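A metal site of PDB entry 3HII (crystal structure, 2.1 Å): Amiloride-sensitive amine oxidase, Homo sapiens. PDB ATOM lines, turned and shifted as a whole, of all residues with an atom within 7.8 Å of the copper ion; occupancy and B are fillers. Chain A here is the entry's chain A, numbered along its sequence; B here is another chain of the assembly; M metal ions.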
ATOM      1  N   ALA A 337      -1.188  -8.745  16.520  1.00  0.00           N
ATOM      2  CA  ALA A 337      -0.582  -9.201  15.292  1.00  0.00           C
ATOM      3  C   ALA A 337      -1.552  -8.847  14.161  1.00  0.00           C
ATOM      4  O   ALA A 337      -2.675  -9.367  14.101  1.00  0.00           O
ATOM      5  CB  ALA A 337      -0.287 -10.722  15.359  1.00  0.00           C
ATOM      6  N   TYR A 339      -2.547  -8.545  10.285  1.00  0.00           N
ATOM      7  CA  TYR A 339      -2.215  -9.301   9.085  1.00  0.00           C
ATOM      8  C   TYR A 339      -2.712  -8.676   7.807  1.00  0.00           C
ATOM      9  O   TYR A 339      -3.660  -7.897   7.808  1.00  0.00           O
ATOM     10  CB  TYR A 339      -2.782 -10.733   9.195  1.00  0.00           C
ATOM     11  CG  TYR A 339      -2.041 -11.538  10.238  1.00  0.00           C
ATOM     12  CD1 TYR A 339      -1.001 -12.385   9.859  1.00  0.00           C
ATOM     13  CD2 TYR A 339      -2.331 -11.405  11.588  1.00  0.00           C
ATOM     14  CE1 TYR A 339      -0.288 -13.089  10.795  1.00  0.00           C
ATOM     15  CE2 TYR A 339      -1.618 -12.120  12.551  1.00  0.00           C
ATOM     16  CZ  TYR A 339      -0.590 -12.955  12.138  1.00  0.00           C
ATOM     17  OH  TYR A 339       0.129 -13.678  13.059  1.00  0.00           O
ATOM     18  N   ASN A 440      -1.059 -20.602  18.395  1.00  0.00           N
ATOM     19  CA  ASN A 440       0.080 -20.939  17.517  1.00  0.00           C
ATOM     20  C   ASN A 440       1.410 -20.373  17.995  1.00  0.00           C
ATOM     21  O   ASN A 440       2.407 -21.089  18.013  1.00  0.00           O
ATOM     22  CB  ASN A 440      -0.193 -20.523  16.061  1.00  0.00           C
ATOM     23  CG  ASN A 440      -0.507 -19.048  15.916  1.00  0.00           C
ATOM     24  OD1 ASN A 440      -1.485 -18.544  16.462  1.00  0.00           O
ATOM     25  ND2 ASN A 440       0.319 -18.336  15.124  1.00  0.00           N
ATOM     26  N   TPQ A 441       1.410 -19.097  18.382  1.00  0.00           N
ATOM     27  CA  TPQ A 441       2.620 -18.392  18.833  1.00  0.00           C
ATOM     28  CB  TPQ A 441       2.442 -16.872  18.641  1.00  0.00           C
ATOM     29  C   TPQ A 441       2.895 -18.534  20.332  1.00  0.00           C
ATOM     30  O   TPQ A 441       1.966 -18.669  21.121  1.00  0.00           O
ATOM     31  C1  TPQ A 441       2.972 -16.372  17.327  1.00  0.00           C
ATOM     32  C2  TPQ A 441       2.085 -15.591  16.437  1.00  0.00           C
ATOM     33  O2  TPQ A 441       0.897 -15.362  16.743  1.00  0.00           O
ATOM     34  C3  TPQ A 441       2.642 -15.086  15.149  1.00  0.00           C
ATOM     35  C4  TPQ A 441       3.980 -15.326  14.799  1.00  0.00           C
ATOM     36  O4  TPQ A 441       4.439 -14.905  13.733  1.00  0.00           O
ATOM     37  C5  TPQ A 441       4.862 -16.099  15.684  1.00  0.00           C
ATOM     38  O5  TPQ A 441       6.054 -16.309  15.363  1.00  0.00           O
ATOM     39  C6  TPQ A 441       4.305 -16.603  16.973  1.00  0.00           C
ATOM     40  N   TYR A 443       4.746 -16.217  23.121  1.00  0.00           N
ATOM     41  CA  TYR A 443       5.483 -15.040  23.517  1.00  0.00           C
ATOM     42  C   TYR A 443       6.165 -15.301  24.863  1.00  0.00           C
ATOM     43  O   TYR A 443       5.596 -15.937  25.761  1.00  0.00           O
ATOM     44  CB  TYR A 443       4.579 -13.817  23.483  1.00  0.00           C
ATOM     45  CG  TYR A 443       3.988 -13.630  22.105  1.00  0.00           C
ATOM     46  CD1 TYR A 443       4.766 -13.190  21.041  1.00  0.00           C
ATOM     47  CD2 TYR A 443       2.662 -13.960  21.837  1.00  0.00           C
ATOM     48  CE1 TYR A 443       4.241 -13.038  19.780  1.00  0.00           C
ATOM     49  CE2 TYR A 443       2.129 -13.814  20.574  1.00  0.00           C
ATOM     50  CZ  TYR A 443       2.912 -13.346  19.551  1.00  0.00           C
ATOM     51  OH  TYR A 443       2.367 -13.202  18.294  1.00  0.00           O
ATOM     52  N   ALA A 461       9.399 -13.499  20.485  1.00  0.00           N
ATOM     53  CA  ALA A 461       8.416 -14.305  19.752  1.00  0.00           C
ATOM     54  C   ALA A 461       9.007 -15.645  19.307  1.00  0.00           C
ATOM     55  O   ALA A 461      10.105 -15.694  18.742  1.00  0.00           O
ATOM     56  CB  ALA A 461       7.906 -13.554  18.545  1.00  0.00           C
ATOM     57  N   THR A 462       8.266 -16.725  19.553  1.00  0.00           N
ATOM     58  CA  THR A 462       8.562 -18.031  18.983  1.00  0.00           C
ATOM     59  C   THR A 462       7.251 -18.838  18.770  1.00  0.00           C
ATOM     60  O   THR A 462       6.172 -18.282  18.817  1.00  0.00           O
ATOM     61  CB  THR A 462       9.642 -18.775  19.825  1.00  0.00           C
ATOM     62  OG1 THR A 462       9.991 -20.002  19.188  1.00  0.00           O
ATOM     63  CG2 THR A 462       9.153 -19.034  21.262  1.00  0.00           C
ATOM     64  N   TYR A 464       4.541 -21.147  16.372  1.00  0.00           N
ATOM     65  CA  TYR A 464       4.126 -21.272  14.964  1.00  0.00           C
ATOM     66  C   TYR A 464       3.551 -19.977  14.401  1.00  0.00           C
ATOM     67  O   TYR A 464       2.759 -19.314  15.081  1.00  0.00           O
ATOM     68  CB  TYR A 464       3.049 -22.354  14.812  1.00  0.00           C
ATOM     69  CG  TYR A 464       3.544 -23.760  15.035  1.00  0.00           C
ATOM     70  CD1 TYR A 464       3.504 -24.342  16.288  1.00  0.00           C
ATOM     71  CD2 TYR A 464       4.049 -24.510  13.964  1.00  0.00           C
ATOM     72  CE1 TYR A 464       3.965 -25.630  16.502  1.00  0.00           C
ATOM     73  CE2 TYR A 464       4.507 -25.802  14.154  1.00  0.00           C
ATOM     74  CZ  TYR A 464       4.456 -26.362  15.430  1.00  0.00           C
ATOM     75  OH  TYR A 464       4.909 -27.635  15.634  1.00  0.00           O
ATOM     76  N   VAL A 465       3.901 -19.646  13.161  1.00  0.00           N
ATOM     77  CA  VAL A 465       3.295 -18.492  12.459  1.00  0.00           C
ATOM     78  C   VAL A 465       1.831 -18.755  12.107  1.00  0.00           C
ATOM     79  O   VAL A 465       1.388 -19.902  12.005  1.00  0.00           O
ATOM     80  CB  VAL A 465       4.071 -18.101  11.150  1.00  0.00           C
ATOM     81  CG1 VAL A 465       5.530 -17.772  11.444  1.00  0.00           C
ATOM     82  CG2 VAL A 465       3.952 -19.189  10.081  1.00  0.00           C
ATOM     83  N   HIS A 466       1.078 -17.664  11.938  1.00  0.00           N
ATOM     84  CA  HIS A 466      -0.283 -17.686  11.423  1.00  0.00           C
ATOM     85  C   HIS A 466      -0.175 -17.756   9.894  1.00  0.00           C
ATOM     86  O   HIS A 466       0.397 -16.859   9.270  1.00  0.00           O
ATOM     87  CB  HIS A 466      -0.993 -16.405  11.857  1.00  0.00           C
ATOM     88  CG  HIS A 466      -2.442 -16.334  11.488  1.00  0.00           C
ATOM     89  ND1 HIS A 466      -3.367 -17.286  11.853  1.00  0.00           N
ATOM     90  CD2 HIS A 466      -3.139 -15.382  10.813  1.00  0.00           C
ATOM     91  CE1 HIS A 466      -4.564 -16.938  11.416  1.00  0.00           C
ATOM     92  NE2 HIS A 466      -4.453 -15.794  10.780  1.00  0.00           N
ATOM     93  N   ASN A 488       1.689 -15.333   6.093  1.00  0.00           N
ATOM     94  CA  ASN A 488       1.160 -13.994   5.896  1.00  0.00           C
ATOM     95  C   ASN A 488       2.015 -12.909   6.541  1.00  0.00           C
ATOM     96  O   ASN A 488       2.508 -13.099   7.666  1.00  0.00           O
ATOM     97  CB  ASN A 488      -0.269 -13.884   6.474  1.00  0.00           C
ATOM     98  CG  ASN A 488      -1.256 -14.797   5.761  1.00  0.00           C
ATOM     99  OD1 ASN A 488      -1.064 -16.012   5.722  1.00  0.00           O
ATOM    100  ND2 ASN A 488      -2.298 -14.223   5.196  1.00  0.00           N
ATOM    101  N   ILE A 489       2.177 -11.799   5.825  1.00  0.00           N
ATOM    102  CA  ILE A 489       2.813 -10.610   6.352  1.00  0.00           C
ATOM    103  C   ILE A 489       1.994 -10.059   7.503  1.00  0.00           C
ATOM    104  O   ILE A 489       0.761 -10.098   7.479  1.00  0.00           O
ATOM    105  CB  ILE A 489       2.964  -9.502   5.264  1.00  0.00           C
ATOM    106  CG1 ILE A 489       3.921  -8.398   5.746  1.00  0.00           C
ATOM    107  CG2 ILE A 489       1.611  -8.927   4.871  1.00  0.00           C
ATOM    108  CD1 ILE A 489       4.242  -7.334   4.670  1.00  0.00           C
ATOM    109  N   HIS A 490       2.682  -9.589   8.537  1.00  0.00           N
ATOM    110  CA  HIS A 490       2.029  -9.007   9.698  1.00  0.00           C
ATOM    111  C   HIS A 490       2.981  -8.157  10.507  1.00  0.00           C
ATOM    112  O   HIS A 490       4.200  -8.223  10.332  1.00  0.00           O
ATOM    113  CB  HIS A 490       1.452 -10.106  10.609  1.00  0.00           C
ATOM    114  CG  HIS A 490       2.478 -11.081  11.104  1.00  0.00           C
ATOM    115  ND1 HIS A 490       3.076 -12.018  10.298  1.00  0.00           N
ATOM    116  CD2 HIS A 490       3.014 -11.255  12.342  1.00  0.00           C
ATOM    117  CE1 HIS A 490       3.936 -12.719  11.006  1.00  0.00           C
ATOM    118  NE2 HIS A 490       3.916 -12.283  12.253  1.00  0.00           N
ATOM    119  N   THR A 491       2.409  -7.367  11.410  1.00  0.00           N
ATOM    120  CA  THR A 491       3.203  -6.601  12.348  1.00  0.00           C
ATOM    121  C   THR A 491       2.773  -6.963  13.755  1.00  0.00           C
ATOM    122  O   THR A 491       1.576  -6.983  14.064  1.00  0.00           O
ATOM    123  CB  THR A 491       3.003  -5.082  12.109  1.00  0.00           C
ATOM    124  OG1 THR A 491       3.444  -4.769  10.782  1.00  0.00           O
ATOM    125  CG2 THR A 491       3.800  -4.256  13.100  1.00  0.00           C
ATOM    126  N   HIS A 492       3.761  -7.283  14.589  1.00  0.00           N
ATOM    127  CA  HIS A 492       3.570  -7.460  16.022  1.00  0.00           C
ATOM    128  C   HIS A 492       3.690  -6.105  16.662  1.00  0.00           C
ATOM    129  O   HIS A 492       4.652  -5.390  16.405  1.00  0.00           O
ATOM    130  CB  HIS A 492       4.665  -8.351  16.634  1.00  0.00           C
ATOM    131  CG  HIS A 492       4.655  -9.756  16.130  1.00  0.00           C
ATOM    132  ND1 HIS A 492       3.850 -10.733  16.663  1.00  0.00           N
ATOM    133  CD2 HIS A 492       5.370 -10.356  15.138  1.00  0.00           C
ATOM    134  CE1 HIS A 492       4.069 -11.872  16.032  1.00  0.00           C
ATOM    135  NE2 HIS A 492       4.981 -11.674  15.108  1.00  0.00           N
ATOM    136  N   PHE A 653       7.534  -5.024  15.632  1.00  0.00           N
ATOM    137  CA  PHE A 653       8.277  -5.243  14.392  1.00  0.00           C
ATOM    138  C   PHE A 653       7.405  -5.842  13.311  1.00  0.00           C
ATOM    139  O   PHE A 653       6.485  -6.625  13.589  1.00  0.00           O
ATOM    140  CB  PHE A 653       9.512  -6.137  14.645  1.00  0.00           C
ATOM    141  CG  PHE A 653       9.197  -7.503  15.228  1.00  0.00           C
ATOM    142  CD1 PHE A 653       9.105  -8.624  14.397  1.00  0.00           C
ATOM    143  CD2 PHE A 653       9.051  -7.680  16.601  1.00  0.00           C
ATOM    144  CE1 PHE A 653       8.838  -9.893  14.928  1.00  0.00           C
ATOM    145  CE2 PHE A 653       8.766  -8.949  17.146  1.00  0.00           C
ATOM    146  CZ  PHE A 653       8.658 -10.060  16.304  1.00  0.00           C
ATOM    147  N   LEU A 654       7.690  -5.442  12.072  1.00  0.00           N
ATOM    148  CA  LEU A 654       7.153  -6.109  10.900  1.00  0.00           C
ATOM    149  C   LEU A 654       7.793  -7.496  10.817  1.00  0.00           C
ATOM    150  O   LEU A 654       9.009  -7.641  10.916  1.00  0.00           O
ATOM    151  CB  LEU A 654       7.496  -5.317   9.616  1.00  0.00           C
ATOM    152  CG  LEU A 654       6.991  -5.888   8.277  1.00  0.00           C
ATOM    153  CD1 LEU A 654       5.472  -5.803   8.138  1.00  0.00           C
ATOM    154  CD2 LEU A 654       7.669  -5.195   7.102  1.00  0.00           C
ATOM    155  N   HIS A 655       6.951  -8.504  10.641  1.00  0.00           N
ATOM    156  CA  HIS A 655       7.397  -9.848  10.379  1.00  0.00           C
ATOM    157  C   HIS A 655       6.926 -10.261   8.973  1.00  0.00           C
ATOM    158  O   HIS A 655       5.724 -10.473   8.724  1.00  0.00           O
ATOM    159  CB  HIS A 655       6.885 -10.789  11.488  1.00  0.00           C
ATOM    160  CG  HIS A 655       7.325 -12.207  11.341  1.00  0.00           C
ATOM    161  ND1 HIS A 655       6.859 -13.210  12.163  1.00  0.00           N
ATOM    162  CD2 HIS A 655       8.169 -12.806  10.467  1.00  0.00           C
ATOM    163  CE1 HIS A 655       7.400 -14.365  11.809  1.00  0.00           C
ATOM    164  NE2 HIS A 655       8.202 -14.143  10.770  1.00  0.00           N
ATOM    165  N   ILE A 656       7.876 -10.335   8.037  1.00  0.00           N
ATOM    166  CA  ILE A 656       7.638 -10.944   6.715  1.00  0.00           C
ATOM    167  C   ILE A 656       8.166 -12.360   6.852  1.00  0.00           C
ATOM    168  O   ILE A 656       9.390 -12.561   6.937  1.00  0.00           O
ATOM    169  CB  ILE A 656       8.405 -10.202   5.585  1.00  0.00           C
ATOM    170  CG1 ILE A 656       7.871  -8.782   5.418  1.00  0.00           C
ATOM    171  CG2 ILE A 656       8.302 -10.974   4.258  1.00  0.00           C
ATOM    172  CD1 ILE A 656       8.770  -7.890   4.538  1.00  0.00           C
ATOM    173  N   PRO A 657       7.266 -13.361   6.927  1.00  0.00           N
ATOM    174  CA  PRO A 657       7.807 -14.707   7.144  1.00  0.00           C
ATOM    175  C   PRO A 657       8.784 -15.185   6.055  1.00  0.00           C
ATOM    176  O   PRO A 657       8.743 -14.727   4.903  1.00  0.00           O
ATOM    177  CB  PRO A 657       6.563 -15.582   7.202  1.00  0.00           C
ATOM    178  CG  PRO A 657       5.484 -14.634   7.716  1.00  0.00           C
ATOM    179  CD  PRO A 657       5.796 -13.338   7.024  1.00  0.00           C
ATOM    180  N   ASP A 661      11.398 -19.733   9.285  1.00  0.00           N
ATOM    181  CA  ASP A 661      10.325 -19.816  10.286  1.00  0.00           C
ATOM    182  C   ASP A 661       9.646 -21.197  10.389  1.00  0.00           C
ATOM    183  O   ASP A 661       8.746 -21.381  11.198  1.00  0.00           O
ATOM    184  CB  ASP A 661       9.223 -18.761  10.008  1.00  0.00           C
ATOM    185  CG  ASP A 661       9.659 -17.352  10.331  1.00  0.00           C
ATOM    186  OD1 ASP A 661      10.331 -17.154  11.359  1.00  0.00           O
ATOM    187  OD2 ASP A 661       9.311 -16.419   9.569  1.00  0.00           O
ATOM    188  N   THR A 665       9.035 -19.878  14.383  1.00  0.00           N
ATOM    189  CA  THR A 665       9.810 -18.658  14.479  1.00  0.00           C
ATOM    190  C   THR A 665      10.803 -18.823  15.622  1.00  0.00           C
ATOM    191  O   THR A 665      10.476 -19.426  16.653  1.00  0.00           O
ATOM    192  CB  THR A 665       8.895 -17.442  14.737  1.00  0.00           C
ATOM    193  OG1 THR A 665       8.014 -17.266  13.617  1.00  0.00           O
ATOM    194  CG2 THR A 665       9.706 -16.162  14.940  1.00  0.00           C
ATOM    195  N   ASN A 670      14.365 -11.597  17.298  1.00  0.00           N
ATOM    196  CA  ASN A 670      12.912 -11.433  17.336  1.00  0.00           C
ATOM    197  C   ASN A 670      12.443 -11.029  18.738  1.00  0.00           C
ATOM    198  O   ASN A 670      11.534 -11.637  19.310  1.00  0.00           O
ATOM    199  CB  ASN A 670      12.187 -12.695  16.855  1.00  0.00           C
ATOM    200  CG  ASN A 670      12.200 -12.849  15.336  1.00  0.00           C
ATOM    201  OD1 ASN A 670      12.224 -11.861  14.607  1.00  0.00           O
ATOM    202  ND2 ASN A 670      12.171 -14.113  14.847  1.00  0.00           N
ATOM    203  N   TYR B 556      13.382  -4.238   6.048  1.00  0.00           N
ATOM    204  CA  TYR B 556      14.115  -5.392   5.527  1.00  0.00           C
ATOM    205  C   TYR B 556      15.216  -4.962   4.561  1.00  0.00           C
ATOM    206  O   TYR B 556      14.931  -4.449   3.483  1.00  0.00           O
ATOM    207  CB  TYR B 556      13.163  -6.409   4.867  1.00  0.00           C
ATOM    208  CG  TYR B 556      12.459  -7.262   5.889  1.00  0.00           C
ATOM    209  CD1 TYR B 556      11.509  -6.714   6.733  1.00  0.00           C
ATOM    210  CD2 TYR B 556      12.779  -8.611   6.045  1.00  0.00           C
ATOM    211  CE1 TYR B 556      10.870  -7.490   7.696  1.00  0.00           C
ATOM    212  CE2 TYR B 556      12.144  -9.390   6.999  1.00  0.00           C
ATOM    213  CZ  TYR B 556      11.198  -8.824   7.827  1.00  0.00           C
ATOM    214  OH  TYR B 556      10.567  -9.589   8.779  1.00  0.00           O
HETATM  215 CU    CU M   1       5.422 -12.913  13.554  1.00  0.00          CU
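NE2 of His 655 sits at hydrogen-bond distance from OD2 of Asp 661 (2.8 Å).
A ring nitrogen (ND1) of His 492 sits close to the side-chain hydroxyl of Tyr 443 (3.3 Å).
The backbone NH (N) of His 492 lies within hydrogen-bond range of the backbone carbonyl oxygen (O) of Phe 653, 3.0 Å away.
The backbone carbonyl oxygen (O) of Asn 488 sits at hydrogen-bond distance from a ring nitrogen (ND1) of His 490, at 2.9 Å.
The side-chain amide nitrogen of Asn 440 lies within hydrogen-bond range of O2 of TPQ 441, 3.4 Å away.
The side-chain hydroxyl (OG1) of Thr 665 sits at hydrogen-bond distance from O5 of TPQ 441, at 2.8 Å.
The side-chain hydroxyl of Tyr 443 sits at hydrogen-bond distance from O2 of TPQ 441 (3.0 Å).
Within 4 Å of the copper ion: TPQ 441, His 490, His 492 and His 655.
ND1 of His 655 binds the copper ion (2.0 Å).
A ring nitrogen (NE2) of His 492 is bound to the copper ion (2.0 Å).
NE2 of His 490 binds the copper ion (2.1 Å).
O4 of TPQ 441 binds the copper ion (2.2 Å).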
